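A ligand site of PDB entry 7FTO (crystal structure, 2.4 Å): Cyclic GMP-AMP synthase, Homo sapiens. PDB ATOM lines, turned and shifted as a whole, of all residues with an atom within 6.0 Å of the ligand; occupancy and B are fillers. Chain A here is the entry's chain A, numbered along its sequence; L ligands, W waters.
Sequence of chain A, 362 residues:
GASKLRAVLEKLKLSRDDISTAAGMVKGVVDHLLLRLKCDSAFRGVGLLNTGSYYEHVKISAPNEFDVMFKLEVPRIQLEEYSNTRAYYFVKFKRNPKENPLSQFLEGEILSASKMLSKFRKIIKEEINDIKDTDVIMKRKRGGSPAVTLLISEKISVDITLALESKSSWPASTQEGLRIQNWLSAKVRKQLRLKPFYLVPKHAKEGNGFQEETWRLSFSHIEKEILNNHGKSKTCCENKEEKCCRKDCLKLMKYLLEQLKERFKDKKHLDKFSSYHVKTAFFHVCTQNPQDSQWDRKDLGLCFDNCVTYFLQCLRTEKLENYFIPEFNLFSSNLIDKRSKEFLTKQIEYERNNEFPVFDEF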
ATOM      1  N   GLU A  56      17.263   0.538  11.200  1.00  0.00           N
ATOM      2  CA  GLU A  56      17.494   1.824  10.546  1.00  0.00           C
ATOM      3  C   GLU A  56      16.796   1.702   9.188  1.00  0.00           C
ATOM      4  O   GLU A  56      17.440   1.562   8.140  1.00  0.00           O
ATOM      5  CB  GLU A  56      19.007   2.143  10.431  1.00  0.00           C
ATOM      6  CG  GLU A  56      19.336   3.569   9.993  1.00  0.00           C
ATOM      7  CD  GLU A  56      19.478   4.608  11.091  1.00  0.00           C
ATOM      8  OE1 GLU A  56      20.189   4.329  12.096  1.00  0.00           O
ATOM      9  OE2 GLU A  56      18.900   5.707  10.944  1.00  0.00           O
ATOM     10  N   LEU A 178      28.492  19.841   9.557  1.00  0.00           N
ATOM     11  CA  LEU A 178      27.499  19.978  10.615  1.00  0.00           C
ATOM     12  C   LEU A 178      27.242  21.501  10.951  1.00  0.00           C
ATOM     13  O   LEU A 178      27.375  21.952  12.090  1.00  0.00           O
ATOM     14  CB  LEU A 178      27.950  19.144  11.823  1.00  0.00           C
ATOM     15  CG  LEU A 178      26.954  18.899  12.958  1.00  0.00           C
ATOM     16  CD1 LEU A 178      25.761  18.004  12.496  1.00  0.00           C
ATOM     17  CD2 LEU A 178      27.688  18.373  14.175  1.00  0.00           C
ATOM     18  N   ILE A 180      25.112  23.588  11.877  1.00  0.00           N
ATOM     19  CA  ILE A 180      23.854  23.679  12.627  1.00  0.00           C
ATOM     20  C   ILE A 180      23.760  24.893  13.604  1.00  0.00           C
ATOM     21  O   ILE A 180      22.675  25.127  14.171  1.00  0.00           O
ATOM     22  CB  ILE A 180      23.608  22.329  13.369  1.00  0.00           C
ATOM     23  CG1 ILE A 180      24.637  22.100  14.501  1.00  0.00           C
ATOM     24  CG2 ILE A 180      23.534  21.142  12.388  1.00  0.00           C
ATOM     25  CD1 ILE A 180      24.331  20.869  15.348  1.00  0.00           C
ATOM     26  N   TRP A 183      20.834  27.249  13.691  1.00  0.00           N
ATOM     27  CA  TRP A 183      19.581  26.510  13.824  1.00  0.00           C
ATOM     28  C   TRP A 183      19.467  25.842  15.247  1.00  0.00           C
ATOM     29  O   TRP A 183      18.629  26.224  16.050  1.00  0.00           O
ATOM     30  CB  TRP A 183      19.472  25.518  12.632  1.00  0.00           C
ATOM     31  CG  TRP A 183      18.532  24.345  12.755  1.00  0.00           C
ATOM     32  CD1 TRP A 183      17.291  24.342  13.330  1.00  0.00           C
ATOM     33  CD2 TRP A 183      18.729  23.035  12.202  1.00  0.00           C
ATOM     34  NE1 TRP A 183      16.724  23.087  13.222  1.00  0.00           N
ATOM     35  CE2 TRP A 183      17.592  22.264  12.544  1.00  0.00           C
ATOM     36  CE3 TRP A 183      19.810  22.401  11.549  1.00  0.00           C
ATOM     37  CZ2 TRP A 183      17.476  20.891  12.200  1.00  0.00           C
ATOM     38  CZ3 TRP A 183      19.692  21.052  11.201  1.00  0.00           C
ATOM     39  CH2 TRP A 183      18.532  20.316  11.511  1.00  0.00           C
ATOM     40  N   ARG A 216      35.336   4.689   4.626  1.00  0.00           N
ATOM     41  CA  ARG A 216      34.577   5.938   4.514  1.00  0.00           C
ATOM     42  C   ARG A 216      34.065   6.332   5.887  1.00  0.00           C
ATOM     43  O   ARG A 216      33.511   5.484   6.600  1.00  0.00           O
ATOM     44  CB  ARG A 216      33.401   5.743   3.524  1.00  0.00           C
ATOM     45  CG  ARG A 216      32.546   6.991   3.296  1.00  0.00           C
ATOM     46  CD  ARG A 216      31.190   6.686   2.694  1.00  0.00           C
ATOM     47  NE  ARG A 216      30.332   5.787   3.493  1.00  0.00           N
ATOM     48  CZ  ARG A 216      29.493   6.175   4.469  1.00  0.00           C
ATOM     49  NH1 ARG A 216      29.413   7.457   4.813  1.00  0.00           N
ATOM     50  NH2 ARG A 216      28.747   5.279   5.099  1.00  0.00           N
ATOM     51  N   LEU A 217      34.223   7.630   6.237  1.00  0.00           N
ATOM     52  CA  LEU A 217      33.744   8.242   7.468  1.00  0.00           C
ATOM     53  C   LEU A 217      32.209   8.249   7.439  1.00  0.00           C
ATOM     54  O   LEU A 217      31.615   8.685   6.442  1.00  0.00           O
ATOM     55  CB  LEU A 217      34.199   9.701   7.581  1.00  0.00           C
ATOM     56  CG  LEU A 217      35.643  10.050   7.839  1.00  0.00           C
ATOM     57  CD1 LEU A 217      35.766  11.572   8.085  1.00  0.00           C
ATOM     58  CD2 LEU A 217      36.208   9.296   9.049  1.00  0.00           C
ATOM     59  N   SER A 218      31.592   7.822   8.566  1.00  0.00           N
ATOM     60  CA  SER A 218      30.150   7.667   8.746  1.00  0.00           C
ATOM     61  C   SER A 218      29.651   8.414   9.971  1.00  0.00           C
ATOM     62  O   SER A 218      30.198   8.252  11.056  1.00  0.00           O
ATOM     63  CB  SER A 218      29.811   6.191   8.896  1.00  0.00           C
ATOM     64  OG  SER A 218      28.447   5.953   8.588  1.00  0.00           O
ATOM     65  N   PHE A 219      28.588   9.219   9.788  1.00  0.00           N
ATOM     66  CA  PHE A 219      27.953   9.945  10.897  1.00  0.00           C
ATOM     67  C   PHE A 219      26.438   9.661  10.975  1.00  0.00           C
ATOM     68  O   PHE A 219      25.690  10.480  11.513  1.00  0.00           O
ATOM     69  CB  PHE A 219      28.235  11.452  10.764  1.00  0.00           C
ATOM     70  CG  PHE A 219      29.702  11.776  10.808  1.00  0.00           C
ATOM     71  CD1 PHE A 219      30.373  11.888  12.029  1.00  0.00           C
ATOM     72  CD2 PHE A 219      30.434  11.961   9.628  1.00  0.00           C
ATOM     73  CE1 PHE A 219      31.739  12.151  12.066  1.00  0.00           C
ATOM     74  CE2 PHE A 219      31.804  12.242   9.664  1.00  0.00           C
ATOM     75  CZ  PHE A 219      32.457  12.310  10.883  1.00  0.00           C
ATOM     76  N   SER A 220      25.998   8.510  10.470  1.00  0.00           N
ATOM     77  CA  SER A 220      24.586   8.103  10.448  1.00  0.00           C
ATOM     78  C   SER A 220      23.950   8.082  11.839  1.00  0.00           C
ATOM     79  O   SER A 220      22.750   8.331  11.955  1.00  0.00           O
ATOM     80  CB  SER A 220      24.387   6.776   9.712  1.00  0.00           C
ATOM     81  OG  SER A 220      25.024   5.732  10.423  1.00  0.00           O
ATOM     82  N   HIS A 221      24.762   7.792  12.877  1.00  0.00           N
ATOM     83  CA  HIS A 221      24.342   7.728  14.273  1.00  0.00           C
ATOM     84  C   HIS A 221      23.920   9.120  14.858  1.00  0.00           C
ATOM     85  O   HIS A 221      23.298   9.171  15.890  1.00  0.00           O
ATOM     86  CB  HIS A 221      25.477   7.096  15.119  1.00  0.00           C
ATOM     87  CG  HIS A 221      26.731   7.938  15.177  1.00  0.00           C
ATOM     88  ND1 HIS A 221      27.537   8.138  14.069  1.00  0.00           N
ATOM     89  CD2 HIS A 221      27.261   8.626  16.225  1.00  0.00           C
ATOM     90  CE1 HIS A 221      28.518   8.925  14.471  1.00  0.00           C
ATOM     91  NE2 HIS A 221      28.389   9.239  15.760  1.00  0.00           N
ATOM     92  N   ILE A 222      24.321  10.226  14.232  1.00  0.00           N
ATOM     93  CA  ILE A 222      24.000  11.591  14.686  1.00  0.00           C
ATOM     94  C   ILE A 222      22.550  11.955  14.275  1.00  0.00           C
ATOM     95  O   ILE A 222      21.954  12.843  14.890  1.00  0.00           O
ATOM     96  CB  ILE A 222      25.056  12.609  14.145  1.00  0.00           C
ATOM     97  CG1 ILE A 222      26.531  12.169  14.429  1.00  0.00           C
ATOM     98  CG2 ILE A 222      24.799  14.055  14.626  1.00  0.00           C
ATOM     99  CD1 ILE A 222      26.963  12.198  15.944  1.00  0.00           C
ATOM    100  N   GLU A 223      21.999  11.312  13.211  1.00  0.00           N
ATOM    101  CA  GLU A 223      20.650  11.602  12.716  1.00  0.00           C
ATOM    102  C   GLU A 223      19.530  11.537  13.775  1.00  0.00           C
ATOM    103  O   GLU A 223      18.716  12.466  13.832  1.00  0.00           O
ATOM    104  CB  GLU A 223      20.280  10.701  11.545  1.00  0.00           C
ATOM    105  CG  GLU A 223      19.000  11.133  10.841  1.00  0.00           C
ATOM    106  CD  GLU A 223      18.614  10.259   9.668  1.00  0.00           C
ATOM    107  OE1 GLU A 223      19.390   9.345   9.330  1.00  0.00           O
ATOM    108  OE2 GLU A 223      17.524  10.504   9.080  1.00  0.00           O
ATOM    109  N   LYS A 224      19.482  10.458  14.586  1.00  0.00           N
ATOM    110  CA  LYS A 224      18.484  10.288  15.655  1.00  0.00           C
ATOM    111  C   LYS A 224      18.613  11.417  16.679  1.00  0.00           C
ATOM    112  O   LYS A 224      17.614  11.924  17.152  1.00  0.00           O
ATOM    113  CB  LYS A 224      18.609   8.892  16.342  1.00  0.00           C
ATOM    114  CG  LYS A 224      20.002   8.637  16.939  1.00  0.00           C
ATOM    115  CD  LYS A 224      20.070   7.405  17.836  1.00  0.00           C
ATOM    116  CE  LYS A 224      21.300   7.458  18.714  1.00  0.00           C
ATOM    117  NZ  LYS A 224      21.114   8.380  19.864  1.00  0.00           N
ATOM    118  N   ILE A 226      19.475  14.483  16.150  1.00  0.00           N
ATOM    119  CA  ILE A 226      18.891  15.686  15.575  1.00  0.00           C
ATOM    120  C   ILE A 226      17.409  15.542  15.340  1.00  0.00           C
ATOM    121  O   ILE A 226      16.699  16.432  15.768  1.00  0.00           O
ATOM    122  CB  ILE A 226      19.684  16.116  14.341  1.00  0.00           C
ATOM    123  CG1 ILE A 226      21.071  16.577  14.871  1.00  0.00           C
ATOM    124  CG2 ILE A 226      18.939  17.242  13.583  1.00  0.00           C
ATOM    125  CD1 ILE A 226      22.085  16.897  13.954  1.00  0.00           C
ATOM    126  N   TYR A 276      19.776   8.428   1.598  1.00  0.00           N
ATOM    127  CA  TYR A 276      20.917   9.182   2.112  1.00  0.00           C
ATOM    128  C   TYR A 276      21.047  10.548   1.423  1.00  0.00           C
ATOM    129  O   TYR A 276      21.324  11.542   2.095  1.00  0.00           O
ATOM    130  CB  TYR A 276      22.180   8.341   1.945  1.00  0.00           C
ATOM    131  CG  TYR A 276      23.434   9.088   2.324  1.00  0.00           C
ATOM    132  CD1 TYR A 276      23.568   9.697   3.575  1.00  0.00           C
ATOM    133  CD2 TYR A 276      24.514   9.145   1.444  1.00  0.00           C
ATOM    134  CE1 TYR A 276      24.728  10.393   3.925  1.00  0.00           C
ATOM    135  CE2 TYR A 276      25.692   9.790   1.802  1.00  0.00           C
ATOM    136  CZ  TYR A 276      25.796  10.400   3.047  1.00  0.00           C
ATOM    137  OH  TYR A 276      26.941  11.068   3.370  1.00  0.00           O
ATOM    138  N   LYS A 279      18.061  12.598   2.606  1.00  0.00           N
ATOM    139  CA  LYS A 279      18.351  13.058   3.992  1.00  0.00           C
ATOM    140  C   LYS A 279      19.334  14.230   3.960  1.00  0.00           C
ATOM    141  O   LYS A 279      18.997  15.288   4.492  1.00  0.00           O
ATOM    142  CB  LYS A 279      18.996  11.946   4.826  1.00  0.00           C
ATOM    143  CG  LYS A 279      18.082  10.801   5.225  1.00  0.00           C
ATOM    144  CD  LYS A 279      18.879   9.765   6.018  1.00  0.00           C
ATOM    145  CE  LYS A 279      18.005   8.572   6.316  1.00  0.00           C
ATOM    146  NZ  LYS A 279      18.734   7.552   7.114  1.00  0.00           N
ATOM    147  N   THR A 280      20.511  14.049   3.295  1.00  0.00           N
ATOM    148  CA  THR A 280      21.545  15.074   3.144  1.00  0.00           C
ATOM    149  C   THR A 280      20.928  16.353   2.660  1.00  0.00           C
ATOM    150  O   THR A 280      21.061  17.350   3.350  1.00  0.00           O
ATOM    151  CB  THR A 280      22.677  14.650   2.201  1.00  0.00           C
ATOM    152  OG1 THR A 280      23.280  13.488   2.716  1.00  0.00           O
ATOM    153  CG2 THR A 280      23.740  15.705   2.059  1.00  0.00           C
ATOM    154  N   PHE A 283      18.533  18.089   5.230  1.00  0.00           N
ATOM    155  CA  PHE A 283      19.228  18.747   6.336  1.00  0.00           C
ATOM    156  C   PHE A 283      19.886  20.056   5.904  1.00  0.00           C
ATOM    157  O   PHE A 283      20.021  20.957   6.727  1.00  0.00           O
ATOM    158  CB  PHE A 283      20.188  17.808   7.058  1.00  0.00           C
ATOM    159  CG  PHE A 283      19.480  16.836   7.962  1.00  0.00           C
ATOM    160  CD1 PHE A 283      18.832  17.271   9.123  1.00  0.00           C
ATOM    161  CD2 PHE A 283      19.411  15.471   7.639  1.00  0.00           C
ATOM    162  CE1 PHE A 283      18.150  16.368   9.958  1.00  0.00           C
ATOM    163  CE2 PHE A 283      18.727  14.562   8.466  1.00  0.00           C
ATOM    164  CZ  PHE A 283      18.128  15.016   9.639  1.00  0.00           C
ATOM    165  N   ASN A 322      28.353  16.515   1.250  1.00  0.00           N
ATOM    166  CA  ASN A 322      28.212  15.709   2.427  1.00  0.00           C
ATOM    167  C   ASN A 322      27.971  16.668   3.625  1.00  0.00           C
ATOM    168  O   ASN A 322      28.669  17.687   3.774  1.00  0.00           O
ATOM    169  CB  ASN A 322      29.438  14.854   2.608  1.00  0.00           C
ATOM    170  CG  ASN A 322      29.367  13.967   3.815  1.00  0.00           C
ATOM    171  OD1 ASN A 322      28.935  14.355   4.895  1.00  0.00           O
ATOM    172  ND2 ASN A 322      29.843  12.768   3.669  1.00  0.00           N
ATOM    173  N   TYR A 323      26.969  16.336   4.448  1.00  0.00           N
ATOM    174  CA  TYR A 323      26.550  17.213   5.534  1.00  0.00           C
ATOM    175  C   TYR A 323      27.631  17.420   6.587  1.00  0.00           C
ATOM    176  O   TYR A 323      27.643  18.467   7.245  1.00  0.00           O
ATOM    177  CB  TYR A 323      25.228  16.732   6.125  1.00  0.00           C
ATOM    178  CG  TYR A 323      24.494  17.829   6.873  1.00  0.00           C
ATOM    179  CD1 TYR A 323      23.719  18.769   6.207  1.00  0.00           C
ATOM    180  CD2 TYR A 323      24.573  17.910   8.270  1.00  0.00           C
ATOM    181  CE1 TYR A 323      23.098  19.808   6.883  1.00  0.00           C
ATOM    182  CE2 TYR A 323      23.936  18.941   8.956  1.00  0.00           C
ATOM    183  CZ  TYR A 323      23.213  19.893   8.257  1.00  0.00           C
ATOM    184  OH  TYR A 323      22.593  20.913   8.921  1.00  0.00           O
ATOM    185  N   PHE A 324      28.583  16.471   6.700  1.00  0.00           N
ATOM    186  CA  PHE A 324      29.685  16.510   7.670  1.00  0.00           C
ATOM    187  C   PHE A 324      31.017  16.852   7.064  1.00  0.00           C
ATOM    188  O   PHE A 324      31.919  17.231   7.796  1.00  0.00           O
ATOM    189  CB  PHE A 324      29.778  15.159   8.382  1.00  0.00           C
ATOM    190  CG  PHE A 324      28.566  14.911   9.243  1.00  0.00           C
ATOM    191  CD1 PHE A 324      27.343  14.547   8.666  1.00  0.00           C
ATOM    192  CD2 PHE A 324      28.630  15.055  10.624  1.00  0.00           C
ATOM    193  CE1 PHE A 324      26.217  14.384   9.445  1.00  0.00           C
ATOM    194  CE2 PHE A 324      27.492  14.871  11.408  1.00  0.00           C
ATOM    195  CZ  PHE A 324      26.297  14.541  10.799  1.00  0.00           C
HETATM  196  C1  LIG L   1      24.936  10.578   7.763  1.00  0.00           C
HETATM  197  C2  LIG L   1      26.835   9.169   6.914  1.00  0.00           C
HETATM  198  O1  LIG L   1      27.191   8.112   6.352  1.00  0.00           O
HETATM  199  C3  LIG L   1      24.377   8.474   6.734  1.00  0.00           C
HETATM  200  C4  LIG L   1      23.022   8.710   6.961  1.00  0.00           C
HETATM  201  C5  LIG L   1      23.213   6.816   5.978  1.00  0.00           C
HETATM  202  C6  LIG L   1      22.436  14.462   8.372  1.00  0.00           C
HETATM  203  C7  LIG L   1      22.242  15.969  10.395  1.00  0.00           C
HETATM  204  C8  LIG L   1      22.521  14.631   9.767  1.00  0.00           C
HETATM  205  C9  LIG L   1      22.957  13.528  10.494  1.00  0.00           C
HETATM  206  C10 LIG L   1      23.270  12.315   9.943  1.00  0.00           C
HETATM  207  C11 LIG L   1      23.154  12.130   8.568  1.00  0.00           C
HETATM  208  C12 LIG L   1      22.739  13.239   7.794  1.00  0.00           C
HETATM  209  C13 LIG L   1      23.582  10.825   7.981  1.00  0.00           C
HETATM  210  C14 LIG L   1      22.619   9.903   7.560  1.00  0.00           C
HETATM  211  C15 LIG L   1      25.365   9.373   7.178  1.00  0.00           C
HETATM  212  F1  LIG L   1      23.078  13.651  11.826  1.00  0.00           F
HETATM  213  N1  LIG L   1      22.301   7.635   6.455  1.00  0.00           N
HETATM  214  N2  LIG L   1      24.474   7.250   6.129  1.00  0.00           N
HETATM  215  O2  LIG L   1      27.633  10.044   7.320  1.00  0.00           O
HETATM  216 CL1  LIG L   1      22.692  13.120   6.063  1.00  0.00          CL
HETATM  217  O   HOH W   1      27.112  12.367   5.698  1.00  0.00           O
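Water W1 lies within hydrogen-bond range of the side-chain hydroxyl (OH) of Tyr 276 (2.7 Å), the side-chain amide oxygen (OD1) of Asn 322 (2.8 Å) and an oxygen (O2) of the ligand (2.9 Å).
The side-chain amino group (NZ) of Lys 279 lies within salt-bridge range of the side-chain carboxylate (OE1) of Glu 223. The side-chain hydroxyl (OH) of Tyr 323 lies close to the backbone carbonyl oxygen (O) of Phe 283 (3.4 Å). OG1 of Thr 280 sits at hydrogen-bond distance from O of Tyr 276, at 2.8 Å. The side-chain hydroxyl (OH) of Tyr 276 lies within hydrogen-bond range of the side-chain amide nitrogen (ND2) of Asn 322, 3.4 Å away. The side-chain amide oxygen (OD1) of Asn 322 sits at hydrogen-bond distance from the backbone NH (N) of Phe 324, at 2.8 Å. O of Tyr 323 sits at hydrogen-bond distance from N of Leu 178.
An oxygen (O2) of the ligand lies within hydrogen-bond range of the backbone NH (N) of Phe 219 (2.8 Å). NH1 of Arg 216 is in salt-bridge range of O1 of the ligand (2.8 Å). O1 of the ligand sits at hydrogen-bond distance from OG of Ser 218.
O of Ile 222 lies close to F1 of the ligand (3.4 Å). N of Glu 223 sits close to F1 of the ligand. Ser 220 touches the ligand (CB to C3, 3.4 Å). Ile 226 touches the ligand. CE1 of Tyr 276 touches C3 of the ligand, at 3.4 Å. Lys 279 touches the ligand. Thr 280 touches the ligand. CD2 of Phe 283 touches C6 of the ligand (3.3 Å). CD2 of Tyr 323 touches C7 of the ligand, at 3.7 Å. Phe 324 touches the ligand (CZ to F1, 3.5 Å). Hydrophobic or aromatic side chains within 4 Å of the ligand: Phe 219, Ile 222, Ile 226, Tyr 276, Phe 283, Tyr 323 and Phe 324.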
